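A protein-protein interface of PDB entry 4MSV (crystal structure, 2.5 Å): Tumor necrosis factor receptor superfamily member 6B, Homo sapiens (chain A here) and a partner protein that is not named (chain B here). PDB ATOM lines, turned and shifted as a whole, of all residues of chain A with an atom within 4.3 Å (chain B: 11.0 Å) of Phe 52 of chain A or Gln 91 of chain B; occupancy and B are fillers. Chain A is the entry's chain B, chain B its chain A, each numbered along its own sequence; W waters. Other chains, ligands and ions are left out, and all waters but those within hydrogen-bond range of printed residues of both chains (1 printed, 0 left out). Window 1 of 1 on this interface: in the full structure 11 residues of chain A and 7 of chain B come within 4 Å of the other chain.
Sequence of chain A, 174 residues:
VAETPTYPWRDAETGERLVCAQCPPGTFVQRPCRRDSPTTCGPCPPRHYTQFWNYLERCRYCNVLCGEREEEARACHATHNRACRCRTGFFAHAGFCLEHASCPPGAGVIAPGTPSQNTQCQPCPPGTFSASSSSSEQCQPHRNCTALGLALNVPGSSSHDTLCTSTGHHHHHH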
ATOM      1  N   CYS A  23     -17.294 -35.129 -14.130  1.00  0.00           N
ATOM      2  CA  CYS A  23     -16.462 -36.234 -14.521  1.00  0.00           C
ATOM      3  C   CYS A  23     -14.968 -35.875 -14.698  1.00  0.00           C
ATOM      4  O   CYS A  23     -14.637 -34.776 -15.073  1.00  0.00           O
ATOM      5  CB  CYS A  23     -16.993 -36.793 -15.806  1.00  0.00           C
ATOM      6  SG  CYS A  23     -18.580 -37.556 -15.532  1.00  0.00           S
ATOM      7  N   PRO A  25     -10.902 -35.891 -15.957  1.00  0.00           N
ATOM      8  CA  PRO A  25     -10.206 -35.987 -17.223  1.00  0.00           C
ATOM      9  C   PRO A  25     -10.197 -37.418 -17.687  1.00  0.00           C
ATOM     10  O   PRO A  25      -9.887 -38.272 -16.911  1.00  0.00           O
ATOM     11  CB  PRO A  25      -8.781 -35.538 -16.859  1.00  0.00           C
ATOM     12  CG  PRO A  25      -8.961 -34.570 -15.710  1.00  0.00           C
ATOM     13  CD  PRO A  25     -10.141 -35.099 -14.954  1.00  0.00           C
ATOM     14  N   THR A  50     -10.712 -35.656 -22.789  1.00  0.00           N
ATOM     15  CA  THR A  50     -11.136 -34.578 -21.923  1.00  0.00           C
ATOM     16  C   THR A  50      -9.989 -34.345 -20.963  1.00  0.00           C
ATOM     17  O   THR A  50      -9.413 -35.265 -20.344  1.00  0.00           O
ATOM     18  CB  THR A  50     -12.481 -34.836 -21.244  1.00  0.00           C
ATOM     19  OG1 THR A  50     -12.466 -36.037 -20.483  1.00  0.00           O
ATOM     20  CG2 THR A  50     -13.575 -34.989 -22.315  1.00  0.00           C
ATOM     21  N   GLN A  51      -9.569 -33.116 -20.924  1.00  0.00           N
ATOM     22  CA  GLN A  51      -8.343 -32.809 -20.219  1.00  0.00           C
ATOM     23  C   GLN A  51      -8.648 -32.284 -18.810  1.00  0.00           C
ATOM     24  O   GLN A  51      -7.791 -32.294 -17.970  1.00  0.00           O
ATOM     25  CB  GLN A  51      -7.582 -31.782 -21.021  1.00  0.00           C
ATOM     26  CG  GLN A  51      -6.170 -31.530 -20.577  1.00  0.00           C
ATOM     27  CD  GLN A  51      -5.571 -30.350 -21.344  1.00  0.00           C
ATOM     28  OE1 GLN A  51      -6.261 -29.531 -21.984  1.00  0.00           O
ATOM     29  NE2 GLN A  51      -4.298 -30.254 -21.280  1.00  0.00           N
ATOM     30  N   PHE A  52      -9.863 -31.846 -18.575  1.00  0.00           N
ATOM     31  CA  PHE A  52     -10.216 -31.213 -17.324  1.00  0.00           C
ATOM     32  C   PHE A  52     -11.458 -31.870 -16.784  1.00  0.00           C
ATOM     33  O   PHE A  52     -12.212 -32.532 -17.501  1.00  0.00           O
ATOM     34  CB  PHE A  52     -10.480 -29.698 -17.529  1.00  0.00           C
ATOM     35  CG  PHE A  52      -9.274 -28.957 -18.033  1.00  0.00           C
ATOM     36  CD1 PHE A  52      -8.112 -28.913 -17.269  1.00  0.00           C
ATOM     37  CD2 PHE A  52      -9.266 -28.373 -19.311  1.00  0.00           C
ATOM     38  CE1 PHE A  52      -6.990 -28.269 -17.752  1.00  0.00           C
ATOM     39  CE2 PHE A  52      -8.146 -27.736 -19.798  1.00  0.00           C
ATOM     40  CZ  PHE A  52      -7.006 -27.681 -19.026  1.00  0.00           C
ATOM     41  N   TRP A  53     -11.689 -31.655 -15.507  1.00  0.00           N
ATOM     42  CA  TRP A  53     -13.016 -31.937 -14.978  1.00  0.00           C
ATOM     43  C   TRP A  53     -14.057 -31.270 -15.904  1.00  0.00           C
ATOM     44  O   TRP A  53     -13.889 -30.147 -16.284  1.00  0.00           O
ATOM     45  CB  TRP A  53     -13.135 -31.483 -13.506  1.00  0.00           C
ATOM     46  CG  TRP A  53     -12.295 -32.359 -12.572  1.00  0.00           C
ATOM     47  CD1 TRP A  53     -10.972 -32.197 -12.239  1.00  0.00           C
ATOM     48  CD2 TRP A  53     -12.726 -33.552 -11.907  1.00  0.00           C
ATOM     49  NE1 TRP A  53     -10.570 -33.208 -11.389  1.00  0.00           N
ATOM     50  CE2 TRP A  53     -11.624 -34.051 -11.176  1.00  0.00           C
ATOM     51  CE3 TRP A  53     -13.936 -34.241 -11.855  1.00  0.00           C
ATOM     52  CZ2 TRP A  53     -11.700 -35.220 -10.416  1.00  0.00           C
ATOM     53  CZ3 TRP A  53     -14.017 -35.404 -11.093  1.00  0.00           C
ATOM     54  CH2 TRP A  53     -12.905 -35.872 -10.376  1.00  0.00           C
ATOM     55  N   ASN A  54     -15.114 -31.986 -16.239  1.00  0.00           N
ATOM     56  CA  ASN A  54     -16.126 -31.513 -17.126  1.00  0.00           C
ATOM     57  C   ASN A  54     -17.499 -32.070 -16.876  1.00  0.00           C
ATOM     58  O   ASN A  54     -17.650 -33.022 -16.116  1.00  0.00           O
ATOM     59  CB  ASN A  54     -15.705 -31.931 -18.490  1.00  0.00           C
ATOM     60  CG  ASN A  54     -15.799 -33.403 -18.717  1.00  0.00           C
ATOM     61  OD1 ASN A  54     -16.776 -33.866 -19.300  1.00  0.00           O
ATOM     62  ND2 ASN A  54     -14.731 -34.121 -18.442  1.00  0.00           N
ATOM     63  N   ARG A  60     -14.185 -34.607 -26.627  1.00  0.00           N
ATOM     64  CA  ARG A  60     -13.711 -33.783 -27.681  1.00  0.00           C
ATOM     65  C   ARG A  60     -12.808 -34.576 -28.552  1.00  0.00           C
ATOM     66  O   ARG A  60     -11.999 -35.330 -28.063  1.00  0.00           O
ATOM     67  CB  ARG A  60     -12.867 -32.668 -27.073  1.00  0.00           C
ATOM     68  CG  ARG A  60     -13.697 -31.702 -26.323  1.00  0.00           C
ATOM     69  CD  ARG A  60     -12.880 -30.857 -25.399  1.00  0.00           C
ATOM     70  NE  ARG A  60     -12.210 -29.677 -25.925  1.00  0.00           N
ATOM     71  CZ  ARG A  60     -12.730 -28.458 -26.008  1.00  0.00           C
ATOM     72  NH1 ARG A  60     -11.928 -27.491 -26.372  1.00  0.00           N
ATOM     73  NH2 ARG A  60     -14.005 -28.185 -25.728  1.00  0.00           N
ATOM     74  N   TYR B  83     -15.772 -18.425 -31.976  1.00  0.00           N
ATOM     75  CA  TYR B  83     -15.615 -19.495 -30.989  1.00  0.00           C
ATOM     76  C   TYR B  83     -16.760 -19.612 -29.984  1.00  0.00           C
ATOM     77  O   TYR B  83     -17.644 -18.735 -29.841  1.00  0.00           O
ATOM     78  CB  TYR B  83     -14.271 -19.438 -30.299  1.00  0.00           C
ATOM     79  CG  TYR B  83     -14.070 -18.296 -29.377  1.00  0.00           C
ATOM     80  CD1 TYR B  83     -13.633 -17.059 -29.837  1.00  0.00           C
ATOM     81  CD2 TYR B  83     -14.333 -18.428 -28.024  1.00  0.00           C
ATOM     82  CE1 TYR B  83     -13.507 -15.975 -28.979  1.00  0.00           C
ATOM     83  CE2 TYR B  83     -14.154 -17.353 -27.141  1.00  0.00           C
ATOM     84  CZ  TYR B  83     -13.740 -16.137 -27.616  1.00  0.00           C
ATOM     85  OH  TYR B  83     -13.599 -15.086 -26.728  1.00  0.00           O
ATOM     86  N   MET B  84     -16.802 -20.805 -29.386  1.00  0.00           N
ATOM     87  CA  MET B  84     -17.857 -21.167 -28.512  1.00  0.00           C
ATOM     88  C   MET B  84     -17.277 -21.464 -27.163  1.00  0.00           C
ATOM     89  O   MET B  84     -16.153 -22.019 -27.039  1.00  0.00           O
ATOM     90  CB  MET B  84     -18.559 -22.376 -29.012  1.00  0.00           C
ATOM     91  CG  MET B  84     -19.885 -22.530 -28.335  1.00  0.00           C
ATOM     92  SD  MET B  84     -19.812 -23.758 -27.009  1.00  0.00           S
ATOM     93  CE  MET B  84     -19.705 -25.223 -28.065  1.00  0.00           C
ATOM     94  N   ARG B  85     -18.051 -21.079 -26.170  1.00  0.00           N
ATOM     95  CA  ARG B  85     -17.776 -21.377 -24.771  1.00  0.00           C
ATOM     96  C   ARG B  85     -19.087 -21.752 -24.073  1.00  0.00           C
ATOM     97  O   ARG B  85     -20.140 -21.178 -24.333  1.00  0.00           O
ATOM     98  CB  ARG B  85     -17.134 -20.150 -24.184  1.00  0.00           C
ATOM     99  CG  ARG B  85     -16.745 -20.153 -22.707  1.00  0.00           C
ATOM    100  CD  ARG B  85     -16.408 -18.687 -22.248  1.00  0.00           C
ATOM    101  NE  ARG B  85     -15.288 -18.086 -23.021  1.00  0.00           N
ATOM    102  CZ  ARG B  85     -14.118 -17.682 -22.539  1.00  0.00           C
ATOM    103  NH1 ARG B  85     -13.863 -17.729 -21.236  1.00  0.00           N
ATOM    104  NH2 ARG B  85     -13.190 -17.208 -23.371  1.00  0.00           N
ATOM    105  N   ASN B  86     -19.045 -22.786 -23.265  1.00  0.00           N
ATOM    106  CA  ASN B  86     -20.081 -23.017 -22.266  1.00  0.00           C
ATOM    107  C   ASN B  86     -19.499 -23.499 -20.919  1.00  0.00           C
ATOM    108  O   ASN B  86     -18.266 -23.647 -20.778  1.00  0.00           O
ATOM    109  CB  ASN B  86     -21.108 -23.950 -22.802  1.00  0.00           C
ATOM    110  CG  ASN B  86     -20.575 -25.342 -22.955  1.00  0.00           C
ATOM    111  OD1 ASN B  86     -19.707 -25.756 -22.244  1.00  0.00           O
ATOM    112  ND2 ASN B  86     -21.102 -26.050 -23.862  1.00  0.00           N
ATOM    113  N   SER B  87     -20.371 -23.712 -19.935  1.00  0.00           N
ATOM    114  CA  SER B  87     -19.939 -24.098 -18.536  1.00  0.00           C
ATOM    115  C   SER B  87     -19.395 -25.548 -18.414  1.00  0.00           C
ATOM    116  O   SER B  87     -18.729 -25.888 -17.429  1.00  0.00           O
ATOM    117  CB  SER B  87     -21.097 -24.023 -17.576  1.00  0.00           C
ATOM    118  OG  SER B  87     -21.837 -22.880 -17.719  1.00  0.00           O
ATOM    119  N   LYS B  88     -19.680 -26.384 -19.397  1.00  0.00           N
ATOM    120  CA  LYS B  88     -19.354 -27.795 -19.304  1.00  0.00           C
ATOM    121  C   LYS B  88     -17.917 -28.126 -19.475  1.00  0.00           C
ATOM    122  O   LYS B  88     -17.529 -29.240 -19.227  1.00  0.00           O
ATOM    123  CB  LYS B  88     -20.082 -28.548 -20.391  1.00  0.00           C
ATOM    124  CG  LYS B  88     -21.561 -28.385 -20.260  1.00  0.00           C
ATOM    125  CD  LYS B  88     -22.295 -28.968 -21.449  1.00  0.00           C
ATOM    126  CE  LYS B  88     -23.789 -28.661 -21.285  1.00  0.00           C
ATOM    127  NZ  LYS B  88     -24.509 -29.753 -21.959  1.00  0.00           N
ATOM    128  N   TYR B  89     -17.124 -27.211 -19.979  1.00  0.00           N
ATOM    129  CA  TYR B  89     -15.713 -27.494 -20.158  1.00  0.00           C
ATOM    130  C   TYR B  89     -15.032 -26.165 -19.984  1.00  0.00           C
ATOM    131  O   TYR B  89     -15.584 -25.158 -20.273  1.00  0.00           O
ATOM    132  CB  TYR B  89     -15.429 -28.141 -21.524  1.00  0.00           C
ATOM    133  CG  TYR B  89     -14.094 -28.791 -21.686  1.00  0.00           C
ATOM    134  CD1 TYR B  89     -13.808 -30.038 -21.114  1.00  0.00           C
ATOM    135  CD2 TYR B  89     -13.119 -28.218 -22.428  1.00  0.00           C
ATOM    136  CE1 TYR B  89     -12.538 -30.652 -21.276  1.00  0.00           C
ATOM    137  CE2 TYR B  89     -11.899 -28.845 -22.654  1.00  0.00           C
ATOM    138  CZ  TYR B  89     -11.605 -30.049 -22.051  1.00  0.00           C
ATOM    139  OH  TYR B  89     -10.412 -30.627 -22.273  1.00  0.00           O
ATOM    140  N   PRO B  90     -13.850 -26.150 -19.440  1.00  0.00           N
ATOM    141  CA  PRO B  90     -13.293 -24.846 -19.148  1.00  0.00           C
ATOM    142  C   PRO B  90     -12.347 -24.350 -20.240  1.00  0.00           C
ATOM    143  O   PRO B  90     -11.338 -23.759 -19.979  1.00  0.00           O
ATOM    144  CB  PRO B  90     -12.560 -25.094 -17.824  1.00  0.00           C
ATOM    145  CG  PRO B  90     -12.058 -26.456 -17.953  1.00  0.00           C
ATOM    146  CD  PRO B  90     -13.139 -27.215 -18.730  1.00  0.00           C
ATOM    147  N   GLN B  91     -12.687 -24.613 -21.474  1.00  0.00           N
ATOM    148  CA  GLN B  91     -11.874 -24.239 -22.541  1.00  0.00           C
ATOM    149  C   GLN B  91     -12.702 -24.096 -23.814  1.00  0.00           C
ATOM    150  O   GLN B  91     -13.713 -24.794 -24.055  1.00  0.00           O
ATOM    151  CB  GLN B  91     -10.770 -25.206 -22.651  1.00  0.00           C
ATOM    152  CG  GLN B  91      -9.941 -24.948 -23.855  1.00  0.00           C
ATOM    153  CD  GLN B  91      -8.591 -25.557 -23.709  1.00  0.00           C
ATOM    154  OE1 GLN B  91      -7.833 -25.214 -22.760  1.00  0.00           O
ATOM    155  NE2 GLN B  91      -8.255 -26.481 -24.653  1.00  0.00           N
ATOM    156  N   ASP B  92     -12.301 -23.117 -24.606  1.00  0.00           N
ATOM    157  CA  ASP B  92     -13.110 -22.677 -25.722  1.00  0.00           C
ATOM    158  C   ASP B  92     -13.007 -23.681 -26.839  1.00  0.00           C
ATOM    159  O   ASP B  92     -12.069 -24.466 -26.849  1.00  0.00           O
ATOM    160  CB  ASP B  92     -12.574 -21.338 -26.207  1.00  0.00           C
ATOM    161  CG  ASP B  92     -12.711 -20.231 -25.145  1.00  0.00           C
ATOM    162  OD1 ASP B  92     -13.649 -20.381 -24.300  1.00  0.00           O
ATOM    163  OD2 ASP B  92     -11.863 -19.263 -25.183  1.00  0.00           O
ATOM    164  N   LEU B  93     -13.968 -23.663 -27.763  1.00  0.00           N
ATOM    165  CA  LEU B  93     -13.842 -24.401 -29.043  1.00  0.00           C
ATOM    166  C   LEU B  93     -13.922 -23.453 -30.268  1.00  0.00           C
ATOM    167  O   LEU B  93     -14.876 -22.672 -30.399  1.00  0.00           O
ATOM    168  CB  LEU B  93     -14.937 -25.479 -29.099  1.00  0.00           C
ATOM    169  CG  LEU B  93     -14.916 -26.442 -30.302  1.00  0.00           C
ATOM    170  CD1 LEU B  93     -13.736 -27.430 -30.387  1.00  0.00           C
ATOM    171  CD2 LEU B  93     -16.211 -27.233 -30.266  1.00  0.00           C
ATOM    172  N   VAL B  94     -12.937 -23.484 -31.147  1.00  0.00           N
ATOM    173  CA  VAL B  94     -12.970 -22.632 -32.360  1.00  0.00           C
ATOM    174  C   VAL B  94     -13.834 -23.252 -33.423  1.00  0.00           C
ATOM    175  O   VAL B  94     -13.646 -24.352 -33.785  1.00  0.00           O
ATOM    176  CB  VAL B  94     -11.577 -22.467 -32.953  1.00  0.00           C
ATOM    177  CG1 VAL B  94     -11.602 -21.603 -34.216  1.00  0.00           C
ATOM    178  CG2 VAL B  94     -10.671 -21.764 -31.930  1.00  0.00           C
ATOM    179  N   MET B  95     -14.799 -22.521 -33.931  1.00  0.00           N
ATOM    180  CA  MET B  95     -15.720 -23.078 -34.880  1.00  0.00           C
ATOM    181  C   MET B  95     -15.228 -22.724 -36.267  1.00  0.00           C
ATOM    182  O   MET B  95     -15.326 -23.548 -37.165  1.00  0.00           O
ATOM    183  CB  MET B  95     -17.076 -22.513 -34.612  1.00  0.00           C
ATOM    184  CG  MET B  95     -17.660 -22.958 -33.255  1.00  0.00           C
ATOM    185  SD  MET B  95     -18.910 -21.752 -32.691  1.00  0.00           S
ATOM    186  CE  MET B  95     -20.227 -21.831 -33.936  1.00  0.00           C
ATOM    187  N   ASP B 126     -24.917 -22.396 -24.896  1.00  0.00           N
ATOM    188  CA  ASP B 126     -23.696 -22.024 -25.628  1.00  0.00           C
ATOM    189  C   ASP B 126     -23.642 -20.508 -25.855  1.00  0.00           C
ATOM    190  O   ASP B 126     -24.659 -19.840 -26.132  1.00  0.00           O
ATOM    191  CB  ASP B 126     -23.590 -22.765 -26.957  1.00  0.00           C
ATOM    192  CG  ASP B 126     -23.477 -24.259 -26.787  1.00  0.00           C
ATOM    193  OD1 ASP B 126     -23.267 -24.669 -25.613  1.00  0.00           O
ATOM    194  OD2 ASP B 126     -23.608 -25.024 -27.802  1.00  0.00           O
ATOM    195  N   HIS B 127     -22.440 -19.984 -25.713  1.00  0.00           N
ATOM    196  CA  HIS B 127     -22.131 -18.568 -25.892  1.00  0.00           C
ATOM    197  C   HIS B 127     -21.115 -18.519 -27.035  1.00  0.00           C
ATOM    198  O   HIS B 127     -20.072 -19.184 -26.983  1.00  0.00           O
ATOM    199  CB  HIS B 127     -21.440 -17.976 -24.634  1.00  0.00           C
ATOM    200  CG  HIS B 127     -22.340 -17.790 -23.457  1.00  0.00           C
ATOM    201  ND1 HIS B 127     -23.145 -18.794 -22.961  1.00  0.00           N
ATOM    202  CD2 HIS B 127     -22.546 -16.714 -22.657  1.00  0.00           C
ATOM    203  CE1 HIS B 127     -23.821 -18.331 -21.922  1.00  0.00           C
ATOM    204  NE2 HIS B 127     -23.484 -17.070 -21.727  1.00  0.00           N
ATOM    205  N   TYR B 129     -18.620 -16.138 -29.630  1.00  0.00           N
ATOM    206  CA  TYR B 129     -17.840 -14.918 -29.568  1.00  0.00           C
ATOM    207  C   TYR B 129     -16.983 -14.803 -30.813  1.00  0.00           C
ATOM    208  O   TYR B 129     -16.674 -15.808 -31.480  1.00  0.00           O
ATOM    209  CB  TYR B 129     -16.872 -14.943 -28.360  1.00  0.00           C
ATOM    210  CG  TYR B 129     -17.543 -15.050 -27.020  1.00  0.00           C
ATOM    211  CD1 TYR B 129     -17.985 -13.904 -26.356  1.00  0.00           C
ATOM    212  CD2 TYR B 129     -17.690 -16.294 -26.358  1.00  0.00           C
ATOM    213  CE1 TYR B 129     -18.559 -13.964 -25.108  1.00  0.00           C
ATOM    214  CE2 TYR B 129     -18.272 -16.369 -25.097  1.00  0.00           C
ATOM    215  CZ  TYR B 129     -18.719 -15.196 -24.499  1.00  0.00           C
ATOM    216  OH  TYR B 129     -19.340 -15.221 -23.296  1.00  0.00           O
HETATM  217  O   HOH W   1      -8.547 -29.262 -23.221  1.00  0.00           O
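O of Phe 52 of chain A lies within hydrogen-bond range of ND2 of Asn 54 of chain A, 3.1 Å away. N of Cys 23 of chain A lies within hydrogen-bond range of O of Asn 54 of chain A (2.9 Å). OD1 of Asn 86 of chain B lies within hydrogen-bond range of N of Lys 88 of chain B. NH2 of Arg 85 of chain B is in salt-bridge range of OD2 of Asp 92 of chain B (3.0 Å).
Phe 52 of chain A touches three residues of chain B. Of the printed residues of chain A, Gln 91 of chain B touches Phe 52 and Arg 60. No residue of chain B comes within 4 Å of Pro 25 of chain A. Of chain B, only Tyr 89 (3.0 Å) comes within 4 Å of Gln 51 of chain A. Of the printed residues of chain B, Asn 54 of chain A touches Lys 88 (3.3 Å) and Tyr 89 (3.8 Å). Printed residues of chain A within 4 Å of Tyr 89 of chain B: Thr 50 (3.96 Å), Gln 51 (3.0 Å), Phe 52 (3.9 Å), Asn 54 (3.8 Å) and Arg 60 (3.4 Å). Of the printed residues of chain A, Lys 88 of chain B touches Asn 54. Printed residues of chain A within 4 Å of Asp 92 of chain B: Arg 60 (3.1 Å). Of the printed residues of chain A, Pro 90 of chain B touches Phe 52 and Trp 53. Of the printed residues of chain B, Arg 60 of chain A touches Tyr 89, Gln 91 and Asp 92. His 127 of chain B touches none of the printed residues of chain A.
Water W1 lies within hydrogen-bond range of OH of Tyr 89 of chain B (2.5 Å), OE1 of Gln 51 of chain A (2.6 Å) and NE2 of Gln 91 of chain B (3.1 Å).
Among the printed residues, pairs that only touch across the chains: Asn 54 of chain A with Lys 88 of chain B (3.3 Å), Arg 60 of chain A with Tyr 89 of chain B (3.4 Å), Phe 52 of chain A with Pro 90 of chain B (3.6 Å), Asn 54 of chain A with Tyr 89 of chain B (3.8 Å), Arg 60 of chain A with Gln 91 of chain B (3.8 Å), Trp 53 of chain A with Pro 90 of chain B (3.9 Å), Phe 52 of chain A with Tyr 89 of chain B (3.9 Å), Phe 52 of chain A with Gln 91 of chain B (3.9 Å) and Thr 50 of chain A with Tyr 89 of chain B (3.96 Å).
NH1 of Arg 60 of chain A sits at hydrogen-bond distance from O of Asp 92 of chain B, 3.1 Å away. N of Gln 51 of chain A lies within hydrogen-bond range of OH of Tyr 89 of chain B (3.0 Å).
Of the 16 printed residues of chain B, 5 touch a printed residue of chain A. Hydrophobic or aromatic side chains of chain B that line the printed part of chain A: Tyr 89 and Pro 90. Printed residues of chain A that touch a printed residue of chain B: Thr 50, Gln 51, Phe 52, Trp 53, Asn 54 and Arg 60.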
